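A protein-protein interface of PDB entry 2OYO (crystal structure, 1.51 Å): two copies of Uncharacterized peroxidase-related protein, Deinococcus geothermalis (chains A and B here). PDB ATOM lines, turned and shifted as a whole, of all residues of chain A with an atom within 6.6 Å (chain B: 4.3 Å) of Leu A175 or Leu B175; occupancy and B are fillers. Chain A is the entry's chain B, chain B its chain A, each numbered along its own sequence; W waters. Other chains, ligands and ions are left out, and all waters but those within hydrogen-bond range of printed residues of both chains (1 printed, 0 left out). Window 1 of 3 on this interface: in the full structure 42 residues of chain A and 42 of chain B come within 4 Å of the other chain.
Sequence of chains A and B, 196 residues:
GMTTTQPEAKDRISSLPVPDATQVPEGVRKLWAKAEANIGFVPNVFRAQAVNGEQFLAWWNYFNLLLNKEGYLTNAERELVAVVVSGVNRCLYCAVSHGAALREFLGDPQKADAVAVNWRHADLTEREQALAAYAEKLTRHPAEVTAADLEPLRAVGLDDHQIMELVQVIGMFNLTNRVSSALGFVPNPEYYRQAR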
ATOM      1  N   GLN A  49     -14.559  -5.226  17.725  1.00  0.00           N
ATOM      2  CA  GLN A  49     -15.241  -6.226  16.941  1.00  0.00           C
ATOM      3  C   GLN A  49     -14.416  -6.753  15.766  1.00  0.00           C
ATOM      4  O   GLN A  49     -14.864  -7.642  15.025  1.00  0.00           O
ATOM      5  CB  GLN A  49     -16.607  -5.670  16.446  1.00  0.00           C
ATOM      6  CG  GLN A  49     -17.602  -6.753  16.072  1.00  0.00           C
ATOM      7  CD  GLN A  49     -18.956  -6.239  15.662  1.00  0.00           C
ATOM      8  OE1 GLN A  49     -19.554  -5.344  16.318  1.00  0.00           O
ATOM      9  NE2 GLN A  49     -19.473  -6.814  14.558  1.00  0.00           N
ATOM     10  N   TRP A  59     -19.673  -8.008   8.096  1.00  0.00           N
ATOM     11  CA  TRP A  59     -20.659  -7.312   8.921  1.00  0.00           C
ATOM     12  C   TRP A  59     -20.709  -5.844   8.576  1.00  0.00           C
ATOM     13  O   TRP A  59     -21.789  -5.271   8.319  1.00  0.00           O
ATOM     14  CB  TRP A  59     -20.290  -7.439  10.429  1.00  0.00           C
ATOM     15  CG  TRP A  59     -21.133  -6.499  11.242  1.00  0.00           C
ATOM     16  CD1 TRP A  59     -22.455  -6.639  11.559  1.00  0.00           C
ATOM     17  CD2 TRP A  59     -20.730  -5.205  11.700  1.00  0.00           C
ATOM     18  NE1 TRP A  59     -22.881  -5.514  12.208  1.00  0.00           N
ATOM     19  CE2 TRP A  59     -21.832  -4.633  12.350  1.00  0.00           C
ATOM     20  CE3 TRP A  59     -19.509  -4.514  11.713  1.00  0.00           C
ATOM     21  CZ2 TRP A  59     -21.783  -3.344  12.946  1.00  0.00           C
ATOM     22  CZ3 TRP A  59     -19.468  -3.226  12.298  1.00  0.00           C
ATOM     23  CH2 TRP A  59     -20.608  -2.670  12.923  1.00  0.00           C
ATOM     24  N   TYR A  62     -22.470  -4.895   5.276  1.00  0.00           N
ATOM     25  CA  TYR A  62     -23.926  -4.929   5.369  1.00  0.00           C
ATOM     26  C   TYR A  62     -24.478  -3.783   6.245  1.00  0.00           C
ATOM     27  O   TYR A  62     -25.444  -3.080   5.869  1.00  0.00           O
ATOM     28  CB  TYR A  62     -24.358  -6.309   5.923  1.00  0.00           C
ATOM     29  CG  TYR A  62     -25.824  -6.550   6.103  1.00  0.00           C
ATOM     30  CD1 TYR A  62     -26.749  -6.003   5.258  1.00  0.00           C
ATOM     31  CD2 TYR A  62     -26.305  -7.375   7.105  1.00  0.00           C
ATOM     32  CE1 TYR A  62     -28.091  -6.257   5.415  1.00  0.00           C
ATOM     33  CE2 TYR A  62     -27.651  -7.625   7.278  1.00  0.00           C
ATOM     34  CZ  TYR A  62     -28.548  -7.064   6.438  1.00  0.00           C
ATOM     35  OH  TYR A  62     -29.891  -7.358   6.599  1.00  0.00           O
ATOM     36  N   LEU A  66     -26.967  -0.745   5.018  1.00  0.00           N
ATOM     37  CA  LEU A  66     -28.333  -0.716   5.539  1.00  0.00           C
ATOM     38  C   LEU A  66     -28.608   0.572   6.357  1.00  0.00           C
ATOM     39  O   LEU A  66     -29.680   1.173   6.249  1.00  0.00           O
ATOM     40  CB  LEU A  66     -28.582  -1.972   6.409  1.00  0.00           C
ATOM     41  CG  LEU A  66     -29.964  -2.251   6.980  1.00  0.00           C
ATOM     42  CD1 LEU A  66     -30.904  -2.563   5.854  1.00  0.00           C
ATOM     43  CD2 LEU A  66     -29.828  -3.374   8.080  1.00  0.00           C
ATOM     44  N   ASN A  89     -33.473  -3.083  24.634  1.00  0.00           N
ATOM     45  CA  ASN A  89     -32.426  -4.052  25.000  1.00  0.00           C
ATOM     46  C   ASN A  89     -31.363  -3.591  25.988  1.00  0.00           C
ATOM     47  O   ASN A  89     -30.585  -4.418  26.479  1.00  0.00           O
ATOM     48  CB  ASN A  89     -31.726  -4.591  23.746  1.00  0.00           C
ATOM     49  CG  ASN A  89     -32.649  -5.483  22.868  1.00  0.00           C
ATOM     50  OD1 ASN A  89     -33.572  -6.146  23.396  1.00  0.00           O
ATOM     51  ND2 ASN A  89     -32.408  -5.479  21.541  1.00  0.00           N
ATOM     52  N   VAL A 167     -37.534  -3.985   8.660  1.00  0.00           N
ATOM     53  CA  VAL A 167     -37.440  -5.231   9.401  1.00  0.00           C
ATOM     54  C   VAL A 167     -35.988  -5.612   9.527  1.00  0.00           C
ATOM     55  O   VAL A 167     -35.558  -6.123  10.560  1.00  0.00           O
ATOM     56  CB  VAL A 167     -38.359  -6.380   8.844  1.00  0.00           C
ATOM     57  CG1 VAL A 167     -39.866  -5.940   8.904  1.00  0.00           C
ATOM     58  CG2 VAL A 167     -37.899  -6.909   7.448  1.00  0.00           C
ATOM     59  N   GLN A 168     -35.193  -5.353   8.493  1.00  0.00           N
ATOM     60  CA  GLN A 168     -33.740  -5.563   8.590  1.00  0.00           C
ATOM     61  C   GLN A 168     -33.041  -4.647   9.599  1.00  0.00           C
ATOM     62  O   GLN A 168     -32.180  -5.067  10.341  1.00  0.00           O
ATOM     63  CB  GLN A 168     -33.081  -5.345   7.229  1.00  0.00           C
ATOM     64  CG  GLN A 168     -33.353  -6.368   6.183  1.00  0.00           C
ATOM     65  CD  GLN A 168     -32.691  -5.962   4.900  1.00  0.00           C
ATOM     66  OE1 GLN A 168     -31.501  -6.203   4.684  1.00  0.00           O
ATOM     67  NE2 GLN A 168     -33.412  -5.244   4.081  1.00  0.00           N
ATOM     68  N   ILE A 170     -34.466  -3.332  12.272  1.00  0.00           N
ATOM     69  CA  ILE A 170     -34.819  -3.844  13.618  1.00  0.00           C
ATOM     70  C   ILE A 170     -34.000  -5.089  13.918  1.00  0.00           C
ATOM     71  O   ILE A 170     -33.406  -5.241  15.000  1.00  0.00           O
ATOM     72  CB  ILE A 170     -36.338  -4.116  13.749  1.00  0.00           C
ATOM     73  CG1 ILE A 170     -37.139  -2.823  13.586  1.00  0.00           C
ATOM     74  CG2 ILE A 170     -36.682  -4.879  15.092  1.00  0.00           C
ATOM     75  CD1 ILE A 170     -38.604  -3.047  13.141  1.00  0.00           C
ATOM     76  N   GLY A 171     -33.922  -5.994  12.940  1.00  0.00           N
ATOM     77  CA  GLY A 171     -33.067  -7.164  13.091  1.00  0.00           C
ATOM     78  C   GLY A 171     -31.646  -6.857  13.431  1.00  0.00           C
ATOM     79  O   GLY A 171     -31.005  -7.520  14.272  1.00  0.00           O
ATOM     80  N   MET A 172     -31.085  -5.937  12.679  1.00  0.00           N
ATOM     81  CA  MET A 172     -29.678  -5.579  12.828  1.00  0.00           C
ATOM     82  C   MET A 172     -29.340  -5.071  14.192  1.00  0.00           C
ATOM     83  O   MET A 172     -28.323  -5.463  14.750  1.00  0.00           O
ATOM     84  CB  MET A 172     -29.272  -4.495  11.770  1.00  0.00           C
ATOM     85  CG  MET A 172     -27.791  -4.095  11.888  1.00  0.00           C
ATOM     86  SD  MET A 172     -26.526  -5.507  11.725  1.00  0.00           S
ATOM     87  CE  MET A 172     -26.315  -5.449   9.841  1.00  0.00           C
ATOM     88  N   PHE A 173     -30.207  -4.230  14.755  1.00  0.00           N
ATOM     89  CA  PHE A 173     -29.977  -3.784  16.149  1.00  0.00           C
ATOM     90  C   PHE A 173     -30.157  -4.903  17.190  1.00  0.00           C
ATOM     91  O   PHE A 173     -29.461  -4.919  18.208  1.00  0.00           O
ATOM     92  CB  PHE A 173     -30.692  -2.435  16.424  1.00  0.00           C
ATOM     93  CG  PHE A 173     -29.967  -1.342  15.758  1.00  0.00           C
ATOM     94  CD1 PHE A 173     -28.738  -0.930  16.254  1.00  0.00           C
ATOM     95  CD2 PHE A 173     -30.382  -0.883  14.541  1.00  0.00           C
ATOM     96  CE1 PHE A 173     -27.976  -0.001  15.567  1.00  0.00           C
ATOM     97  CE2 PHE A 173     -29.623   0.040  13.860  1.00  0.00           C
ATOM     98  CZ  PHE A 173     -28.417   0.463  14.377  1.00  0.00           C
ATOM     99  N   ASN A 174     -31.028  -5.861  16.918  1.00  0.00           N
ATOM    100  CA  ASN A 174     -31.100  -7.052  17.743  1.00  0.00           C
ATOM    101  C   ASN A 174     -29.837  -7.898  17.634  1.00  0.00           C
ATOM    102  O   ASN A 174     -29.447  -8.544  18.594  1.00  0.00           O
ATOM    103  CB  ASN A 174     -32.412  -7.799  17.468  1.00  0.00           C
ATOM    104  CG  ASN A 174     -33.590  -7.129  18.135  1.00  0.00           C
ATOM    105  OD1 ASN A 174     -34.363  -6.346  17.514  1.00  0.00           O
ATOM    106  ND2 ASN A 174     -33.736  -7.392  19.380  1.00  0.00           N
ATOM    107  N   LEU A 175     -29.147  -7.840  16.494  1.00  0.00           N
ATOM    108  CA  LEU A 175     -27.815  -8.475  16.358  1.00  0.00           C
ATOM    109  C   LEU A 175     -26.737  -7.633  17.075  1.00  0.00           C
ATOM    110  O   LEU A 175     -26.015  -8.119  17.957  1.00  0.00           O
ATOM    111  CB  LEU A 175     -27.505  -8.617  14.855  1.00  0.00           C
ATOM    112  CG  LEU A 175     -26.163  -9.222  14.415  1.00  0.00           C
ATOM    113  CD1 LEU A 175     -26.170  -9.645  12.913  1.00  0.00           C
ATOM    114  CD2 LEU A 175     -24.958  -8.341  14.631  1.00  0.00           C
ATOM    115  N   THR A 176     -26.590  -6.367  16.711  1.00  0.00           N
ATOM    116  CA  THR A 176     -25.537  -5.544  17.301  1.00  0.00           C
ATOM    117  C   THR A 176     -25.745  -5.317  18.812  1.00  0.00           C
ATOM    118  O   THR A 176     -24.761  -5.270  19.549  1.00  0.00           O
ATOM    119  CB  THR A 176     -25.366  -4.228  16.560  1.00  0.00           C
ATOM    120  OG1 THR A 176     -26.511  -3.414  16.795  1.00  0.00           O
ATOM    121  CG2 THR A 176     -25.073  -4.483  15.008  1.00  0.00           C
ATOM    122  N   ASN A 177     -26.989  -5.128  19.282  1.00  0.00           N
ATOM    123  CA  ASN A 177     -27.187  -5.005  20.756  1.00  0.00           C
ATOM    124  C   ASN A 177     -26.613  -6.234  21.467  1.00  0.00           C
ATOM    125  O   ASN A 177     -25.976  -6.114  22.516  1.00  0.00           O
ATOM    126  CB  ASN A 177     -28.670  -4.864  21.129  1.00  0.00           C
ATOM    127  CG  ASN A 177     -29.298  -3.564  20.731  1.00  0.00           C
ATOM    128  OD1 ASN A 177     -30.567  -3.430  20.821  1.00  0.00           O
ATOM    129  ND2 ASN A 177     -28.476  -2.579  20.270  1.00  0.00           N
ATOM    130  N   ARG A 178     -26.841  -7.428  20.898  1.00  0.00           N
ATOM    131  CA  ARG A 178     -26.340  -8.670  21.509  1.00  0.00           C
ATOM    132  C   ARG A 178     -24.875  -8.826  21.446  1.00  0.00           C
ATOM    133  O   ARG A 178     -24.287  -9.200  22.431  1.00  0.00           O
ATOM    134  CB  ARG A 178     -27.060  -9.876  20.928  1.00  0.00           C
ATOM    135  CG  ARG A 178     -28.497  -9.889  21.447  1.00  0.00           C
ATOM    136  CD  ARG A 178     -29.392 -10.942  20.812  1.00  0.00           C
ATOM    137  NE  ARG A 178     -30.675 -11.058  21.505  1.00  0.00           N
ATOM    138  CZ  ARG A 178     -31.731 -10.248  21.323  1.00  0.00           C
ATOM    139  NH1 ARG A 178     -31.703  -9.323  20.399  1.00  0.00           N
ATOM    140  NH2 ARG A 178     -32.837 -10.428  22.022  1.00  0.00           N
ATOM    141  N   VAL A 179     -24.260  -8.560  20.314  1.00  0.00           N
ATOM    142  CA  VAL A 179     -22.799  -8.674  20.206  1.00  0.00           C
ATOM    143  C   VAL A 179     -22.137  -7.650  21.149  1.00  0.00           C
ATOM    144  O   VAL A 179     -21.248  -7.987  21.906  1.00  0.00           O
ATOM    145  CB  VAL A 179     -22.299  -8.441  18.756  1.00  0.00           C
ATOM    146  CG1 VAL A 179     -20.779  -8.364  18.732  1.00  0.00           C
ATOM    147  CG2 VAL A 179     -22.840  -9.508  17.836  1.00  0.00           C
ATOM    148  N   SER A 180     -22.605  -6.412  21.135  1.00  0.00           N
ATOM    149  CA  SER A 180     -21.958  -5.344  21.921  1.00  0.00           C
ATOM    150  C   SER A 180     -22.150  -5.589  23.417  1.00  0.00           C
ATOM    151  O   SER A 180     -21.214  -5.373  24.194  1.00  0.00           O
ATOM    152  CB  SER A 180     -22.490  -3.930  21.557  1.00  0.00           C
ATOM    153  OG  SER A 180     -22.285  -3.626  20.187  1.00  0.00           O
ATOM    154  N   TYR B  62     -22.509 -11.807   4.363  1.00  0.00           N
ATOM    155  CA  TYR B  62     -22.132 -11.965   5.779  1.00  0.00           C
ATOM    156  C   TYR B  62     -22.662 -13.289   6.328  1.00  0.00           C
ATOM    157  O   TYR B  62     -21.912 -14.061   6.934  1.00  0.00           O
ATOM    158  CB  TYR B  62     -22.673 -10.790   6.559  1.00  0.00           C
ATOM    159  CG  TYR B  62     -22.431 -10.768   8.046  1.00  0.00           C
ATOM    160  CD1 TYR B  62     -21.249 -11.287   8.597  1.00  0.00           C
ATOM    161  CD2 TYR B  62     -23.357 -10.174   8.918  1.00  0.00           C
ATOM    162  CE1 TYR B  62     -21.041 -11.237   9.961  1.00  0.00           C
ATOM    163  CE2 TYR B  62     -23.155 -10.124  10.276  1.00  0.00           C
ATOM    164  CZ  TYR B  62     -22.007 -10.636  10.808  1.00  0.00           C
ATOM    165  OH  TYR B  62     -21.783 -10.600  12.182  1.00  0.00           O
ATOM    166  N   GLY B 171     -26.477 -13.403  17.522  1.00  0.00           N
ATOM    167  CA  GLY B 171     -27.029 -12.124  17.035  1.00  0.00           C
ATOM    168  C   GLY B 171     -27.670 -12.286  15.691  1.00  0.00           C
ATOM    169  O   GLY B 171     -28.774 -11.774  15.427  1.00  0.00           O
ATOM    170  N   MET B 172     -27.001 -13.041  14.828  1.00  0.00           N
ATOM    171  CA  MET B 172     -27.528 -13.268  13.485  1.00  0.00           C
ATOM    172  C   MET B 172     -28.921 -13.920  13.406  1.00  0.00           C
ATOM    173  O   MET B 172     -29.807 -13.520  12.620  1.00  0.00           O
ATOM    174  CB  MET B 172     -26.528 -14.115  12.660  1.00  0.00           C
ATOM    175  CG  MET B 172     -27.025 -14.280  11.180  1.00  0.00           C
ATOM    176  SD  MET B 172     -27.465 -12.739  10.124  1.00  0.00           S
ATOM    177  CE  MET B 172     -25.764 -12.490   9.472  1.00  0.00           C
ATOM    178  N   PHE B 173     -29.094 -14.948  14.215  1.00  0.00           N
ATOM    179  CA  PHE B 173     -30.418 -15.585  14.334  1.00  0.00           C
ATOM    180  C   PHE B 173     -31.471 -14.706  14.981  1.00  0.00           C
ATOM    181  O   PHE B 173     -32.637 -14.749  14.603  1.00  0.00           O
ATOM    182  CB  PHE B 173     -30.239 -17.008  14.905  1.00  0.00           C
ATOM    183  CG  PHE B 173     -29.694 -17.909  13.847  1.00  0.00           C
ATOM    184  CD1 PHE B 173     -30.517 -18.267  12.790  1.00  0.00           C
ATOM    185  CD2 PHE B 173     -28.344 -18.223  13.773  1.00  0.00           C
ATOM    186  CE1 PHE B 173     -30.037 -18.996  11.739  1.00  0.00           C
ATOM    187  CE2 PHE B 173     -27.861 -18.945  12.681  1.00  0.00           C
ATOM    188  CZ  PHE B 173     -28.703 -19.324  11.699  1.00  0.00           C
ATOM    189  N   ASN B 174     -31.040 -13.823  15.881  1.00  0.00           N
ATOM    190  CA  ASN B 174     -31.939 -12.746  16.347  1.00  0.00           C
ATOM    191  C   ASN B 174     -32.320 -11.768  15.271  1.00  0.00           C
ATOM    192  O   ASN B 174     -33.448 -11.269  15.253  1.00  0.00           O
ATOM    193  CB  ASN B 174     -31.392 -12.121  17.650  1.00  0.00           C
ATOM    194  CG  ASN B 174     -31.635 -13.055  18.859  1.00  0.00           C
ATOM    195  OD1 ASN B 174     -32.768 -13.082  19.371  1.00  0.00           O
ATOM    196  ND2 ASN B 174     -30.621 -13.889  19.244  1.00  0.00           N
ATOM    197  N   LEU B 175     -31.419 -11.558  14.322  1.00  0.00           N
ATOM    198  CA  LEU B 175     -31.762 -10.815  13.101  1.00  0.00           C
ATOM    199  C   LEU B 175     -32.644 -11.608  12.148  1.00  0.00           C
ATOM    200  O   LEU B 175     -33.740 -11.156  11.815  1.00  0.00           O
ATOM    201  CB  LEU B 175     -30.476 -10.334  12.397  1.00  0.00           C
ATOM    202  CG  LEU B 175     -30.595  -9.483  11.127  1.00  0.00           C
ATOM    203  CD1 LEU B 175     -29.256  -8.802  10.782  1.00  0.00           C
ATOM    204  CD2 LEU B 175     -31.066 -10.327   9.977  1.00  0.00           C
ATOM    205  N   THR B 176     -32.210 -12.803  11.736  1.00  0.00           N
ATOM    206  CA  THR B 176     -32.997 -13.551  10.770  1.00  0.00           C
ATOM    207  C   THR B 176     -34.336 -14.015  11.314  1.00  0.00           C
ATOM    208  O   THR B 176     -35.293 -14.003  10.584  1.00  0.00           O
ATOM    209  CB  THR B 176     -32.230 -14.748  10.180  1.00  0.00           C
ATOM    210  OG1 THR B 176     -31.960 -15.705  11.211  1.00  0.00           O
ATOM    211  CG2 THR B 176     -30.903 -14.259   9.493  1.00  0.00           C
ATOM    212  N   ASN B 177     -34.427 -14.431  12.574  1.00  0.00           N
ATOM    213  CA  ASN B 177     -35.736 -14.776  13.173  1.00  0.00           C
ATOM    214  C   ASN B 177     -36.750 -13.639  13.028  1.00  0.00           C
ATOM    215  O   ASN B 177     -37.895 -13.845  12.668  1.00  0.00           O
ATOM    216  CB  ASN B 177     -35.591 -15.174  14.636  1.00  0.00           C
ATOM    217  CG  ASN B 177     -34.912 -16.496  14.840  1.00  0.00           C
ATOM    218  OD1 ASN B 177     -34.592 -17.281  13.865  1.00  0.00           O
ATOM    219  ND2 ASN B 177     -34.626 -16.764  16.093  1.00  0.00           N
ATOM    220  N   ARG B 178     -36.284 -12.441  13.269  1.00  0.00           N
ATOM    221  CA  ARG B 178     -37.109 -11.261  13.170  1.00  0.00           C
ATOM    222  C   ARG B 178     -37.527 -10.915  11.781  1.00  0.00           C
ATOM    223  O   ARG B 178     -38.701 -10.704  11.562  1.00  0.00           O
ATOM    224  CB  ARG B 178     -36.489 -10.081  13.925  1.00  0.00           C
ATOM    225  CG  ARG B 178     -36.583 -10.286  15.429  1.00  0.00           C
ATOM    226  CD  ARG B 178     -35.932  -9.194  16.243  1.00  0.00           C
ATOM    227  NE  ARG B 178     -36.186  -9.449  17.671  1.00  0.00           N
ATOM    228  CZ  ARG B 178     -35.550 -10.330  18.452  1.00  0.00           C
ATOM    229  NH1 ARG B 178     -34.528 -11.099  18.022  1.00  0.00           N
ATOM    230  NH2 ARG B 178     -36.001 -10.451  19.676  1.00  0.00           N
ATOM    231  N   VAL B 179     -36.611 -10.922  10.823  1.00  0.00           N
ATOM    232  CA  VAL B 179     -36.952 -10.630   9.439  1.00  0.00           C
ATOM    233  C   VAL B 179     -37.935 -11.711   8.943  1.00  0.00           C
ATOM    234  O   VAL B 179     -38.990 -11.413   8.378  1.00  0.00           O
ATOM    235  CB  VAL B 179     -35.709 -10.560   8.505  1.00  0.00           C
ATOM    236  CG1 VAL B 179     -36.147 -10.485   6.994  1.00  0.00           C
ATOM    237  CG2 VAL B 179     -34.811  -9.358   8.912  1.00  0.00           C
HETATM  238  O   HOH W   1     -35.363 -12.751  21.409  1.00  0.00           O
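The side-chain amide nitrogen of Asn A89 lies close to the side-chain amide nitrogen of Asn A174 (3.2 Å). The backbone carbonyl oxygen (O) of Met A172 lies close to the side-chain hydroxyl (OG1) of Thr A176. OG1 of Thr B176 sits at hydrogen-bond distance from O of Met B172, at 3.4 Å. The side-chain amide oxygen (OD1) of Asn A174 lies close to the backbone carbonyl oxygen (O) of Ile A170 (2.9 Å). OD1 of Asn B174 lies within hydrogen-bond range of NH1 of Arg B178, at 3.0 Å. OH of Tyr A62 sits at hydrogen-bond distance from OE1 of Gln A168 (2.8 Å).
CG2 of Val B179 touches O of Val A167, 3.7 Å away. Gln A168 touches Val B179. Gly A171 touches Leu B175 (O to CB, 3.4 Å). Met A172 touches Leu B175 (CA to CD1, 3.8 Å). CD of Arg B178 touches OD1 of Asn A174 (3.5 Å). Leu A175 touches Gly B171. Met B172 touches Leu A175 (CA to CD1, 3.9 Å). Leu B175 touches Leu A175 (CD1 to CD1, 3.8 Å). CG of Asn B174 touches NE of Arg A178, at 3.5 Å. Arg B178 touches Arg A178 (NH2 to NH2, 3.9 Å).
Of chain B, only Gly B171, Met B172 and Leu B175 come within 4 Å of Leu A175. Of chain A, only Gly A171 (3.4 Å), Met A172 (3.8 Å) and Leu A175 (3.8 Å) come within 4 Å of Leu B175. Of the printed residues of chain A, Gly B171 touches Leu A175 (3.5 Å). Of the printed residues of chain B, Met A172 touches Leu B175. The nearest residue of chain B that does not touch Leu A175 is Tyr B62 (4.03 Å). The nearest residue of chain A that does not touch Leu B175 is Tyr A62 (4.03 Å).
Hydrophobic or aromatic side chains of chain B within 4 Å of the printed part of chain A: Tyr B62, Leu B175 and Val B179. Among the printed residues, 11 pairs touch across the chains. Among the printed residues, no Asp or Glu carboxylate lies within 4 Å of a Lys or Arg side-chain nitrogen of the other chain.
Gly A171 touches Leu B175, and with the chains exchanged Leu A175 touches Gly B171. Met A172 touches Leu B175, and with the chains exchanged Leu A175 touches Met B172. Asn A174 touches Arg B178, and with the chains exchanged Arg A178 touches Asn B174. Leu B175 touches its own counterpart, Leu A175. Positions printed for both chains: 62, 171, 172, 173, 174, 175, 176, 177, 178 and 179.
Water W1 lies within hydrogen-bond range of the guanidinium group of Arg B178, the side-chain amide oxygen of Asn B174 and the guanidinium group of Arg A178.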
